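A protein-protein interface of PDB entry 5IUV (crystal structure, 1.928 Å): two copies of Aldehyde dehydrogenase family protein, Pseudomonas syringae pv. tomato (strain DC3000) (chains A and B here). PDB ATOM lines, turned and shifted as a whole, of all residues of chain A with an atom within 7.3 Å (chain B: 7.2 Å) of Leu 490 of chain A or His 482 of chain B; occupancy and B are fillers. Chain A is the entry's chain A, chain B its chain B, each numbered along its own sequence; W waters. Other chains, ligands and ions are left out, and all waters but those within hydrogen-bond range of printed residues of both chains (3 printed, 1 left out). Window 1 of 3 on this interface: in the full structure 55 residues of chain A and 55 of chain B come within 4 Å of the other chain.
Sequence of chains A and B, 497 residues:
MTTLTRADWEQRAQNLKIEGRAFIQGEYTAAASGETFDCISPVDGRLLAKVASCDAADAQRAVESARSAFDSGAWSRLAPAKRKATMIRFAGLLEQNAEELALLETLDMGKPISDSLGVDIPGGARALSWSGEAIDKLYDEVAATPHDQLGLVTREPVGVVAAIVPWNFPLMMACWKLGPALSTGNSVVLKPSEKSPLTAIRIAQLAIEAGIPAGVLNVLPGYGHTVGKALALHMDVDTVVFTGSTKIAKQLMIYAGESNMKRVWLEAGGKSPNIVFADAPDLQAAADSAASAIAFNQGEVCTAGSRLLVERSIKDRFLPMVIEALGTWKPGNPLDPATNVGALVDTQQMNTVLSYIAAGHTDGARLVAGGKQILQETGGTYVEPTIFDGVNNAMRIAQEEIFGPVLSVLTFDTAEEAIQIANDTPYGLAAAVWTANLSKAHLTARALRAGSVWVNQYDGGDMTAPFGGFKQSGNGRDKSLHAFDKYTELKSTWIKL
O of Thr 154 of chain A lies within hydrogen-bond range of N of Lys 491 of chain A, at 2.8 Å. The backbone carbonyl oxygen of Glu 141 of chain A sits at hydrogen-bond distance from the backbone NH of Val 153 of chain A (2.8 Å).
CG of Pro 466 of chain B touches CG1 of Val 153 of chain A (3.6 Å). Glu 489 of chain A touches Phe 470 of chain B. Lys 491 of chain A touches Ala 450 of chain B. Ala 465 of chain B touches Ser 492 of chain A.
The backbone carbonyl oxygen (O) of Gly 469 of chain B lies close to the side-chain carboxylate (OE1) of Glu 489 of chain A (3.5 Å). The backbone carbonyl oxygen (O) of Gly 451 of chain B sits at hydrogen-bond distance from the backbone NH (N) of Ser 492 of chain A (2.8 Å). The guanidinium group of Arg 477 of chain B is in salt-bridge range of the side-chain carboxylate of Glu 489 of chain A (3.0 Å). The side-chain carboxylate (OE1) of Glu 141 of chain A sits at hydrogen-bond distance from a ring nitrogen (NE2) of His 482 of chain B, 2.7 Å away. The side-chain hydroxyl of Ser 492 of chain A lies within hydrogen-bond range of the backbone carbonyl oxygen of Pro 466 of chain B (2.7 Å). The backbone carbonyl oxygen (O) of Leu 490 of chain A is in hydrogen-bond range of the guanidinium group (NH2) of Arg 477 of chain B, at 2.8 Å.
Of the 13 printed residues of chain A, 7 touch a printed residue of chain B. Hydrophobic or aromatic side chains of chain A within 4 Å of the printed part of chain B: Val 153 and Leu 490. Of the 25 printed residues of chain B, 9 touch a printed residue of chain A. Along chain B the printed residues that touch a printed residue of chain A span positions 450 to 482. Among the printed residues, 16 pairs touch across the chains. Among the printed residues, Asp or Glu carboxylates within 4 Å of a Lys or Arg side-chain nitrogen of the other chain: Glu 489 of chain A with Arg 477 of chain B (3.0 Å).
Printed residues of chain A within 4 Å of Ser 452 of chain B: Ser 492. Of the printed residues of chain A, Arg 477 of chain B touches Glu 489 (3.0 Å) and Leu 490 (2.8 Å). Ser 480 of chain B touches none of the printed residues of chain A. The nearest residue of chain A that does not touch His 482 of chain B is Val 153 of chain A (4.1 Å).
1 position is printed for both chains.
Water W3 bridges the backbone NH (N) of Gly 476 of chain B (2.9 Å) and the side-chain carboxylate (OE1) of Glu 489 of chain A (3.1 Å). Water W2 lies within hydrogen-bond range of N of Leu 490 of chain A (3.0 Å) and NH2 of Arg 477 of chain B (3.5 Å).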
ATOM      1  N   ASP A 140      35.129 -12.980 -22.505  1.00  0.00           N
ATOM      2  CA  ASP A 140      34.492 -12.081 -23.458  1.00  0.00           C
ATOM      3  C   ASP A 140      34.174 -12.858 -24.740  1.00  0.00           C
ATOM      4  O   ASP A 140      34.107 -14.087 -24.703  1.00  0.00           O
ATOM      5  CB  ASP A 140      35.372 -10.854 -23.707  1.00  0.00           C
ATOM      6  CG  ASP A 140      35.372  -9.890 -22.515  1.00  0.00           C
ATOM      7  OD1 ASP A 140      34.400  -9.924 -21.728  1.00  0.00           O
ATOM      8  OD2 ASP A 140      36.336  -9.107 -22.360  1.00  0.00           O
ATOM      9  N   GLU A 141      33.943 -12.168 -25.856  1.00  0.00           N
ATOM     10  CA  GLU A 141      33.323 -12.840 -27.004  1.00  0.00           C
ATOM     11  C   GLU A 141      34.065 -12.718 -28.332  1.00  0.00           C
ATOM     12  O   GLU A 141      34.765 -11.741 -28.584  1.00  0.00           O
ATOM     13  CB  GLU A 141      31.892 -12.316 -27.198  1.00  0.00           C
ATOM     14  CG  GLU A 141      30.948 -12.672 -26.070  1.00  0.00           C
ATOM     15  CD  GLU A 141      29.689 -11.834 -26.093  1.00  0.00           C
ATOM     16  OE1 GLU A 141      29.790 -10.615 -26.355  1.00  0.00           O
ATOM     17  OE2 GLU A 141      28.598 -12.391 -25.861  1.00  0.00           O
ATOM     18  N   VAL A 153      34.677  -8.971 -29.192  1.00  0.00           N
ATOM     19  CA  VAL A 153      33.798  -8.152 -28.371  1.00  0.00           C
ATOM     20  C   VAL A 153      34.268  -8.281 -26.936  1.00  0.00           C
ATOM     21  O   VAL A 153      34.031  -9.304 -26.297  1.00  0.00           O
ATOM     22  CB  VAL A 153      32.319  -8.587 -28.500  1.00  0.00           C
ATOM     23  CG1 VAL A 153      31.427  -7.718 -27.614  1.00  0.00           C
ATOM     24  CG2 VAL A 153      31.876  -8.519 -29.949  1.00  0.00           C
ATOM     25  N   THR A 154      34.963  -7.259 -26.444  1.00  0.00           N
ATOM     26  CA  THR A 154      35.630  -7.350 -25.152  1.00  0.00           C
ATOM     27  C   THR A 154      35.150  -6.271 -24.194  1.00  0.00           C
ATOM     28  O   THR A 154      34.484  -5.317 -24.602  1.00  0.00           O
ATOM     29  CB  THR A 154      37.161  -7.238 -25.303  1.00  0.00           C
ATOM     30  OG1 THR A 154      37.492  -5.970 -25.878  1.00  0.00           O
ATOM     31  CG2 THR A 154      37.694  -8.349 -26.203  1.00  0.00           C
ATOM     32  N   ARG A 155      35.502  -6.430 -22.922  1.00  0.00           N
ATOM     33  CA  ARG A 155      35.134  -5.474 -21.888  1.00  0.00           C
ATOM     34  C   ARG A 155      36.371  -4.862 -21.253  1.00  0.00           C
ATOM     35  O   ARG A 155      37.345  -5.559 -20.982  1.00  0.00           O
ATOM     36  CB  ARG A 155      34.280  -6.148 -20.814  1.00  0.00           C
ATOM     37  CG  ARG A 155      32.938  -6.620 -21.330  1.00  0.00           C
ATOM     38  CD  ARG A 155      32.114  -7.237 -20.225  1.00  0.00           C
ATOM     39  NE  ARG A 155      30.709  -7.321 -20.597  1.00  0.00           N
ATOM     40  CZ  ARG A 155      29.855  -6.303 -20.529  1.00  0.00           C
ATOM     41  NH1 ARG A 155      30.262  -5.106 -20.104  1.00  0.00           N
ATOM     42  NH2 ARG A 155      28.593  -6.483 -20.891  1.00  0.00           N
ATOM     43  N   GLU A 156      36.324  -3.557 -21.019  1.00  0.00           N
ATOM     44  CA  GLU A 156      37.433  -2.835 -20.415  1.00  0.00           C
ATOM     45  C   GLU A 156      36.907  -1.977 -19.280  1.00  0.00           C
ATOM     46  O   GLU A 156      35.778  -1.509 -19.342  1.00  0.00           O
ATOM     47  CB  GLU A 156      38.136  -1.964 -21.458  1.00  0.00           C
ATOM     48  CG  GLU A 156      38.657  -2.743 -22.660  1.00  0.00           C
ATOM     49  CD  GLU A 156      39.181  -1.838 -23.755  1.00  0.00           C
ATOM     50  OE1 GLU A 156      38.973  -0.610 -23.656  1.00  0.00           O
ATOM     51  OE2 GLU A 156      39.809  -2.357 -24.701  1.00  0.00           O
ATOM     52  N   VAL A 158      35.944   1.156 -17.021  1.00  0.00           N
ATOM     53  CA  VAL A 158      35.544   2.485 -17.455  1.00  0.00           C
ATOM     54  C   VAL A 158      36.582   3.544 -17.070  1.00  0.00           C
ATOM     55  O   VAL A 158      36.726   4.554 -17.763  1.00  0.00           O
ATOM     56  CB  VAL A 158      34.161   2.872 -16.878  1.00  0.00           C
ATOM     57  CG1 VAL A 158      33.086   1.932 -17.415  1.00  0.00           C
ATOM     58  CG2 VAL A 158      34.175   2.846 -15.350  1.00  0.00           C
ATOM     59  N   ASP A 485      29.197  -5.536 -15.051  1.00  0.00           N
ATOM     60  CA  ASP A 485      28.847  -4.778 -16.248  1.00  0.00           C
ATOM     61  C   ASP A 485      28.676  -3.279 -15.979  1.00  0.00           C
ATOM     62  O   ASP A 485      28.747  -2.476 -16.900  1.00  0.00           O
ATOM     63  CB  ASP A 485      27.572  -5.348 -16.881  1.00  0.00           C
ATOM     64  CG  ASP A 485      27.784  -6.737 -17.477  1.00  0.00           C
ATOM     65  OD1 ASP A 485      28.950  -7.124 -17.724  1.00  0.00           O
ATOM     66  OD2 ASP A 485      26.779  -7.440 -17.705  1.00  0.00           O
ATOM     67  N   THR A 488      32.377  -1.607 -16.571  1.00  0.00           N
ATOM     68  CA  THR A 488      33.123  -1.825 -17.801  1.00  0.00           C
ATOM     69  C   THR A 488      32.412  -1.280 -19.038  1.00  0.00           C
ATOM     70  O   THR A 488      31.222  -0.957 -19.000  1.00  0.00           O
ATOM     71  CB  THR A 488      33.418  -3.329 -18.028  1.00  0.00           C
ATOM     72  OG1 THR A 488      32.194  -4.063 -18.079  1.00  0.00           O
ATOM     73  CG2 THR A 488      34.283  -3.892 -16.911  1.00  0.00           C
ATOM     74  N   GLU A 489      33.170  -1.171 -20.127  1.00  0.00           N
ATOM     75  CA  GLU A 489      32.656  -0.741 -21.430  1.00  0.00           C
ATOM     76  C   GLU A 489      32.902  -1.831 -22.455  1.00  0.00           C
ATOM     77  O   GLU A 489      33.977  -2.427 -22.469  1.00  0.00           O
ATOM     78  CB  GLU A 489      33.344   0.543 -21.911  1.00  0.00           C
ATOM     79  CG  GLU A 489      33.023   1.789 -21.125  1.00  0.00           C
ATOM     80  CD  GLU A 489      31.631   2.314 -21.402  1.00  0.00           C
ATOM     81  OE1 GLU A 489      31.088   2.057 -22.500  1.00  0.00           O
ATOM     82  OE2 GLU A 489      31.072   2.986 -20.514  1.00  0.00           O
ATOM     83  N   LEU A 490      31.927  -2.067 -23.323  1.00  0.00           N
ATOM     84  CA  LEU A 490      32.085  -2.993 -24.439  1.00  0.00           C
ATOM     85  C   LEU A 490      32.848  -2.373 -25.614  1.00  0.00           C
ATOM     86  O   LEU A 490      32.608  -1.228 -25.995  1.00  0.00           O
ATOM     87  CB  LEU A 490      30.719  -3.474 -24.919  1.00  0.00           C
ATOM     88  CG  LEU A 490      30.030  -4.529 -24.056  1.00  0.00           C
ATOM     89  CD1 LEU A 490      28.576  -4.676 -24.472  1.00  0.00           C
ATOM     90  CD2 LEU A 490      30.755  -5.861 -24.188  1.00  0.00           C
ATOM     91  N   LYS A 491      33.750  -3.152 -26.196  1.00  0.00           N
ATOM     92  CA  LYS A 491      34.470  -2.725 -27.386  1.00  0.00           C
ATOM     93  C   LYS A 491      34.376  -3.781 -28.468  1.00  0.00           C
ATOM     94  O   LYS A 491      34.628  -4.958 -28.221  1.00  0.00           O
ATOM     95  CB  LYS A 491      35.940  -2.447 -27.073  1.00  0.00           C
ATOM     96  CG  LYS A 491      36.785  -2.179 -28.324  1.00  0.00           C
ATOM     97  CD  LYS A 491      38.247  -1.910 -27.972  1.00  0.00           C
ATOM     98  CE  LYS A 491      38.407  -0.548 -27.306  1.00  0.00           C
ATOM     99  NZ  LYS A 491      39.798  -0.371 -26.801  1.00  0.00           N
ATOM    100  N   SER A 492      34.010  -3.353 -29.667  1.00  0.00           N
ATOM    101  CA  SER A 492      33.993  -4.234 -30.821  1.00  0.00           C
ATOM    102  C   SER A 492      35.218  -3.987 -31.677  1.00  0.00           C
ATOM    103  O   SER A 492      35.306  -2.957 -32.340  1.00  0.00           O
ATOM    104  CB  SER A 492      32.731  -4.014 -31.651  1.00  0.00           C
ATOM    105  OG  SER A 492      31.596  -4.528 -30.989  1.00  0.00           O
ATOM    106  N   TRP B 130      17.423 -10.078 -38.054  1.00  0.00           N
ATOM    107  CA  TRP B 130      18.473 -10.671 -37.214  1.00  0.00           C
ATOM    108  C   TRP B 130      18.025 -10.695 -35.754  1.00  0.00           C
ATOM    109  O   TRP B 130      18.167 -11.700 -35.060  1.00  0.00           O
ATOM    110  CB  TRP B 130      19.786  -9.895 -37.364  1.00  0.00           C
ATOM    111  CG  TRP B 130      21.003 -10.549 -36.757  1.00  0.00           C
ATOM    112  CD1 TRP B 130      21.927 -11.320 -37.405  1.00  0.00           C
ATOM    113  CD2 TRP B 130      21.440 -10.464 -35.392  1.00  0.00           C
ATOM    114  NE1 TRP B 130      22.907 -11.727 -36.528  1.00  0.00           N
ATOM    115  CE2 TRP B 130      22.630 -11.214 -35.287  1.00  0.00           C
ATOM    116  CE3 TRP B 130      20.939  -9.827 -34.250  1.00  0.00           C
ATOM    117  CZ2 TRP B 130      23.329 -11.342 -34.085  1.00  0.00           C
ATOM    118  CZ3 TRP B 130      21.630  -9.965 -33.057  1.00  0.00           C
ATOM    119  CH2 TRP B 130      22.809 -10.715 -32.983  1.00  0.00           C
ATOM    120  N   LEU B 138      18.262 -17.066 -27.267  1.00  0.00           N
ATOM    121  CA  LEU B 138      18.719 -16.491 -26.002  1.00  0.00           C
ATOM    122  C   LEU B 138      18.272 -17.347 -24.822  1.00  0.00           C
ATOM    123  O   LEU B 138      17.138 -17.813 -24.780  1.00  0.00           O
ATOM    124  CB  LEU B 138      18.186 -15.070 -25.842  1.00  0.00           C
ATOM    125  CG  LEU B 138      18.706 -14.053 -26.854  1.00  0.00           C
ATOM    126  CD1 LEU B 138      17.941 -12.746 -26.728  1.00  0.00           C
ATOM    127  CD2 LEU B 138      20.182 -13.834 -26.622  1.00  0.00           C
ATOM    128  N   PRO B 180      15.492  -5.010 -31.532  1.00  0.00           N
ATOM    129  CA  PRO B 180      15.576  -5.566 -30.176  1.00  0.00           C
ATOM    130  C   PRO B 180      14.447  -5.120 -29.240  1.00  0.00           C
ATOM    131  O   PRO B 180      14.043  -5.909 -28.389  1.00  0.00           O
ATOM    132  CB  PRO B 180      16.933  -5.054 -29.667  1.00  0.00           C
ATOM    133  CG  PRO B 180      17.225  -3.848 -30.509  1.00  0.00           C
ATOM    134  CD  PRO B 180      16.647  -4.155 -31.853  1.00  0.00           C
ATOM    135  N   ALA B 450      37.301   3.623 -27.517  1.00  0.00           N
ATOM    136  CA  ALA B 450      36.186   3.764 -28.447  1.00  0.00           C
ATOM    137  C   ALA B 450      35.384   2.474 -28.537  1.00  0.00           C
ATOM    138  O   ALA B 450      35.934   1.386 -28.378  1.00  0.00           O
ATOM    139  CB  ALA B 450      36.693   4.177 -29.825  1.00  0.00           C
ATOM    140  N   GLY B 451      34.085   2.598 -28.798  1.00  0.00           N
ATOM    141  CA  GLY B 451      33.194   1.448 -28.796  1.00  0.00           C
ATOM    142  C   GLY B 451      33.422   0.478 -29.939  1.00  0.00           C
ATOM    143  O   GLY B 451      33.180  -0.722 -29.794  1.00  0.00           O
ATOM    144  N   SER B 452      33.871   1.005 -31.075  1.00  0.00           N
ATOM    145  CA  SER B 452      34.251   0.190 -32.228  1.00  0.00           C
ATOM    146  C   SER B 452      35.674   0.521 -32.638  1.00  0.00           C
ATOM    147  O   SER B 452      36.022   1.692 -32.774  1.00  0.00           O
ATOM    148  CB  SER B 452      33.319   0.430 -33.423  1.00  0.00           C
ATOM    149  OG  SER B 452      31.978   0.080 -33.144  1.00  0.00           O
ATOM    150  N   THR B 464      26.402  -8.729 -35.781  1.00  0.00           N
ATOM    151  CA  THR B 464      26.992  -9.410 -34.626  1.00  0.00           C
ATOM    152  C   THR B 464      27.835  -8.467 -33.760  1.00  0.00           C
ATOM    153  O   THR B 464      28.254  -8.842 -32.663  1.00  0.00           O
ATOM    154  CB  THR B 464      27.881 -10.617 -35.047  1.00  0.00           C
ATOM    155  OG1 THR B 464      29.059 -10.150 -35.723  1.00  0.00           O
ATOM    156  CG2 THR B 464      27.106 -11.571 -35.952  1.00  0.00           C
ATOM    157  N   ALA B 465      28.069  -7.246 -34.242  1.00  0.00           N
ATOM    158  CA  ALA B 465      28.989  -6.318 -33.571  1.00  0.00           C
ATOM    159  C   ALA B 465      28.264  -5.219 -32.809  1.00  0.00           C
ATOM    160  O   ALA B 465      27.614  -4.380 -33.416  1.00  0.00           O
ATOM    161  CB  ALA B 465      29.942  -5.688 -34.582  1.00  0.00           C
ATOM    162  N   PRO B 466      28.379  -5.220 -31.472  1.00  0.00           N
ATOM    163  CA  PRO B 466      27.769  -4.129 -30.709  1.00  0.00           C
ATOM    164  C   PRO B 466      28.395  -2.799 -31.107  1.00  0.00           C
ATOM    165  O   PRO B 466      29.583  -2.743 -31.424  1.00  0.00           O
ATOM    166  CB  PRO B 466      28.064  -4.484 -29.245  1.00  0.00           C
ATOM    167  CG  PRO B 466      29.096  -5.553 -29.281  1.00  0.00           C
ATOM    168  CD  PRO B 466      28.993  -6.243 -30.604  1.00  0.00           C
ATOM    169  N   PHE B 467      27.581  -1.753 -31.103  1.00  0.00           N
ATOM    170  CA  PHE B 467      27.957  -0.451 -31.630  1.00  0.00           C
ATOM    171  C   PHE B 467      27.482   0.609 -30.644  1.00  0.00           C
ATOM    172  O   PHE B 467      26.310   0.643 -30.280  1.00  0.00           O
ATOM    173  CB  PHE B 467      27.333  -0.257 -33.012  1.00  0.00           C
ATOM    174  CG  PHE B 467      27.667   1.057 -33.673  1.00  0.00           C
ATOM    175  CD1 PHE B 467      27.026   2.226 -33.290  1.00  0.00           C
ATOM    176  CD2 PHE B 467      28.585   1.111 -34.712  1.00  0.00           C
ATOM    177  CE1 PHE B 467      27.315   3.427 -33.897  1.00  0.00           C
ATOM    178  CE2 PHE B 467      28.870   2.316 -35.338  1.00  0.00           C
ATOM    179  CZ  PHE B 467      28.229   3.474 -34.927  1.00  0.00           C
ATOM    180  N   GLY B 468      28.395   1.456 -30.189  1.00  0.00           N
ATOM    181  CA  GLY B 468      28.035   2.488 -29.225  1.00  0.00           C
ATOM    182  C   GLY B 468      29.255   3.158 -28.626  1.00  0.00           C
ATOM    183  O   GLY B 468      30.384   2.814 -28.960  1.00  0.00           O
ATOM    184  N   GLY B 469      29.035   4.115 -27.732  1.00  0.00           N
ATOM    185  CA  GLY B 469      30.117   5.001 -27.339  1.00  0.00           C
ATOM    186  C   GLY B 469      30.788   4.741 -26.006  1.00  0.00           C
ATOM    187  O   GLY B 469      30.192   4.169 -25.097  1.00  0.00           O
ATOM    188  N   PHE B 470      32.058   5.132 -25.929  1.00  0.00           N
ATOM    189  CA  PHE B 470      32.733   5.469 -24.675  1.00  0.00           C
ATOM    190  C   PHE B 470      32.435   6.931 -24.375  1.00  0.00           C
ATOM    191  O   PHE B 470      32.155   7.700 -25.299  1.00  0.00           O
ATOM    192  CB  PHE B 470      34.251   5.301 -24.787  1.00  0.00           C
ATOM    193  CG  PHE B 470      34.739   3.887 -24.669  1.00  0.00           C
ATOM    194  CD1 PHE B 470      34.144   2.856 -25.382  1.00  0.00           C
ATOM    195  CD2 PHE B 470      35.833   3.596 -23.863  1.00  0.00           C
ATOM    196  CE1 PHE B 470      34.619   1.555 -25.272  1.00  0.00           C
ATOM    197  CE2 PHE B 470      36.309   2.301 -23.751  1.00  0.00           C
ATOM    198  CZ  PHE B 470      35.701   1.278 -24.461  1.00  0.00           C
ATOM    199  N   GLY B 476      25.604   2.166 -23.584  1.00  0.00           N
ATOM    200  CA  GLY B 476      24.833   1.074 -24.145  1.00  0.00           C
ATOM    201  C   GLY B 476      25.213   0.834 -25.595  1.00  0.00           C
ATOM    202  O   GLY B 476      25.942   1.621 -26.208  1.00  0.00           O
ATOM    203  N   ARG B 477      24.716  -0.264 -26.149  1.00  0.00           N
ATOM    204  CA  ARG B 477      25.117  -0.676 -27.482  1.00  0.00           C
ATOM    205  C   ARG B 477      23.921  -1.061 -28.340  1.00  0.00           C
ATOM    206  O   ARG B 477      22.977  -1.697 -27.858  1.00  0.00           O
ATOM    207  CB  ARG B 477      26.098  -1.854 -27.398  1.00  0.00           C
ATOM    208  CG  ARG B 477      27.381  -1.571 -26.622  1.00  0.00           C
ATOM    209  CD  ARG B 477      28.271  -0.561 -27.334  1.00  0.00           C
ATOM    210  NE  ARG B 477      29.529  -0.308 -26.621  1.00  0.00           N
ATOM    211  CZ  ARG B 477      29.757   0.742 -25.831  1.00  0.00           C
ATOM    212  NH1 ARG B 477      28.814   1.654 -25.630  1.00  0.00           N
ATOM    213  NH2 ARG B 477      30.939   0.890 -25.249  1.00  0.00           N
ATOM    214  N   ASP B 478      23.970  -0.661 -29.607  1.00  0.00           N
ATOM    215  CA  ASP B 478      23.021  -1.110 -30.622  1.00  0.00           C
ATOM    216  C   ASP B 478      23.641  -2.266 -31.400  1.00  0.00           C
ATOM    217  O   ASP B 478      24.866  -2.432 -31.388  1.00  0.00           O
ATOM    218  CB  ASP B 478      22.645   0.031 -31.578  1.00  0.00           C
ATOM    219  CG  ASP B 478      21.668   1.011 -30.961  1.00  0.00           C
ATOM    220  OD1 ASP B 478      20.926   0.611 -30.039  1.00  0.00           O
ATOM    221  OD2 ASP B 478      21.631   2.180 -31.404  1.00  0.00           O
ATOM    222  N   LYS B 479      22.787  -3.040 -32.073  1.00  0.00           N
ATOM    223  CA  LYS B 479      23.159  -4.280 -32.774  1.00  0.00           C
ATOM    224  C   LYS B 479      23.649  -5.350 -31.791  1.00  0.00           C
ATOM    225  O   LYS B 479      23.772  -5.089 -30.598  1.00  0.00           O
ATOM    226  CB  LYS B 479      24.217  -4.015 -33.853  1.00  0.00           C
ATOM    227  CG  LYS B 479      23.855  -2.889 -34.823  1.00  0.00           C
ATOM    228  CD  LYS B 479      24.706  -2.926 -36.092  1.00  0.00           C
ATOM    229  CE  LYS B 479      26.176  -2.675 -35.804  1.00  0.00           C
ATOM    230  NZ  LYS B 479      26.994  -2.836 -37.037  1.00  0.00           N
ATOM    231  N   SER B 480      23.915  -6.553 -32.306  1.00  0.00           N
ATOM    232  CA  SER B 480      24.294  -7.727 -31.502  1.00  0.00           C
ATOM    233  C   SER B 480      23.228  -8.097 -30.472  1.00  0.00           C
ATOM    234  O   SER B 480      22.159  -7.484 -30.408  1.00  0.00           O
ATOM    235  CB  SER B 480      25.644  -7.511 -30.795  1.00  0.00           C
ATOM    236  OG  SER B 480      25.494  -6.863 -29.544  1.00  0.00           O
ATOM    237  N   LEU B 481      23.528  -9.116 -29.672  1.00  0.00           N
ATOM    238  CA  LEU B 481      22.629  -9.546 -28.612  1.00  0.00           C
ATOM    239  C   LEU B 481      22.636  -8.573 -27.441  1.00  0.00           C
ATOM    240  O   LEU B 481      21.676  -8.511 -26.683  1.00  0.00           O
ATOM    241  CB  LEU B 481      23.008 -10.953 -28.132  1.00  0.00           C
ATOM    242  CG  LEU B 481      23.012 -12.024 -29.226  1.00  0.00           C
ATOM    243  CD1 LEU B 481      23.467 -13.356 -28.662  1.00  0.00           C
ATOM    244  CD2 LEU B 481      21.632 -12.148 -29.853  1.00  0.00           C
ATOM    245  N   HIS B 482      23.710  -7.802 -27.301  1.00  0.00           N
ATOM    246  CA  HIS B 482      23.817  -6.846 -26.203  1.00  0.00           C
ATOM    247  C   HIS B 482      22.775  -5.731 -26.295  1.00  0.00           C
ATOM    248  O   HIS B 482      22.441  -5.109 -25.290  1.00  0.00           O
ATOM    249  CB  HIS B 482      25.217  -6.233 -26.160  1.00  0.00           C
ATOM    250  CG  HIS B 482      26.292  -7.226 -25.853  1.00  0.00           C
ATOM    251  ND1 HIS B 482      26.595  -7.618 -24.566  1.00  0.00           N
ATOM    252  CD2 HIS B 482      27.124  -7.921 -26.666  1.00  0.00           C
ATOM    253  CE1 HIS B 482      27.576  -8.504 -24.601  1.00  0.00           C
ATOM    254  NE2 HIS B 482      27.905  -8.713 -25.863  1.00  0.00           N
ATOM    255  N   ALA B 483      22.262  -5.482 -27.495  1.00  0.00           N
ATOM    256  CA  ALA B 483      21.234  -4.457 -27.677  1.00  0.00           C
ATOM    257  C   ALA B 483      19.963  -4.810 -26.914  1.00  0.00           C
ATOM    258  O   ALA B 483      19.235  -3.927 -26.471  1.00  0.00           O
ATOM    259  CB  ALA B 483      20.926  -4.265 -29.156  1.00  0.00           C
ATOM    260  N   PHE B 484      19.706  -6.106 -26.770  1.00  0.00           N
ATOM    261  CA  PHE B 484      18.501  -6.595 -26.097  1.00  0.00           C
ATOM    262  C   PHE B 484      18.456  -6.152 -24.639  1.00  0.00           C
ATOM    263  O   PHE B 484      17.390  -5.907 -24.078  1.00  0.00           O
ATOM    264  CB  PHE B 484      18.431  -8.123 -26.167  1.00  0.00           C
ATOM    265  CG  PHE B 484      17.956  -8.659 -27.492  1.00  0.00           C
ATOM    266  CD1 PHE B 484      18.646  -8.387 -28.662  1.00  0.00           C
ATOM    267  CD2 PHE B 484      16.837  -9.468 -27.560  1.00  0.00           C
ATOM    268  CE1 PHE B 484      18.200  -8.898 -29.881  1.00  0.00           C
ATOM    269  CE2 PHE B 484      16.393  -9.975 -28.771  1.00  0.00           C
ATOM    270  CZ  PHE B 484      17.078  -9.691 -29.926  1.00  0.00           C
ATOM    271  N   ASP B 485      19.627  -6.045 -24.032  1.00  0.00           N
ATOM    272  CA  ASP B 485      19.729  -5.722 -22.619  1.00  0.00           C
ATOM    273  C   ASP B 485      19.235  -4.318 -22.282  1.00  0.00           C
ATOM    274  O   ASP B 485      18.956  -4.038 -21.126  1.00  0.00           O
ATOM    275  CB  ASP B 485      21.174  -5.893 -22.154  1.00  0.00           C
ATOM    276  CG  ASP B 485      21.636  -7.334 -22.232  1.00  0.00           C
ATOM    277  OD1 ASP B 485      20.766  -8.234 -22.279  1.00  0.00           O
ATOM    278  OD2 ASP B 485      22.862  -7.565 -22.249  1.00  0.00           O
ATOM    279  N   LYS B 486      19.118  -3.442 -23.282  1.00  0.00           N
ATOM    280  CA  LYS B 486      18.568  -2.104 -23.049  1.00  0.00           C
ATOM    281  C   LYS B 486      17.042  -2.117 -22.885  1.00  0.00           C
ATOM    282  O   LYS B 486      16.441  -1.123 -22.458  1.00  0.00           O
ATOM    283  CB  LYS B 486      18.950  -1.159 -24.198  1.00  0.00           C
ATOM    284  CG  LYS B 486      20.449  -0.975 -24.378  1.00  0.00           C
ATOM    285  CD  LYS B 486      20.736   0.034 -25.466  1.00  0.00           C
ATOM    286  CE  LYS B 486      20.163  -0.431 -26.788  1.00  0.00           C
ATOM    287  NZ  LYS B 486      20.365   0.603 -27.836  1.00  0.00           N
ATOM    288  N   TYR B 487      16.415  -3.235 -23.230  1.00  0.00           N
ATOM    289  CA  TYR B 487      14.954  -3.292 -23.296  1.00  0.00           C
ATOM    290  C   TYR B 487      14.374  -4.322 -22.336  1.00  0.00           C
ATOM    291  O   TYR B 487      13.188  -4.668 -22.411  1.00  0.00           O
ATOM    292  CB  TYR B 487      14.507  -3.590 -24.734  1.00  0.00           C
ATOM    293  CG  TYR B 487      15.089  -2.611 -25.728  1.00  0.00           C
ATOM    294  CD1 TYR B 487      14.597  -1.311 -25.824  1.00  0.00           C
ATOM    295  CD2 TYR B 487      16.145  -2.974 -26.549  1.00  0.00           C
ATOM    296  CE1 TYR B 487      15.138  -0.404 -26.723  1.00  0.00           C
ATOM    297  CE2 TYR B 487      16.697  -2.073 -27.454  1.00  0.00           C
ATOM    298  CZ  TYR B 487      16.190  -0.794 -27.536  1.00  0.00           C
ATOM    299  OH  TYR B 487      16.737   0.095 -28.435  1.00  0.00           O
HETATM  300  O   HOH W   1      26.260 -11.693 -26.404  1.00  0.00           O
HETATM  301  O   HOH W   2      29.231  -0.939 -22.818  1.00  0.00           O
HETATM  302  O   HOH W   3      28.036   1.634 -22.175  1.00  0.00           O
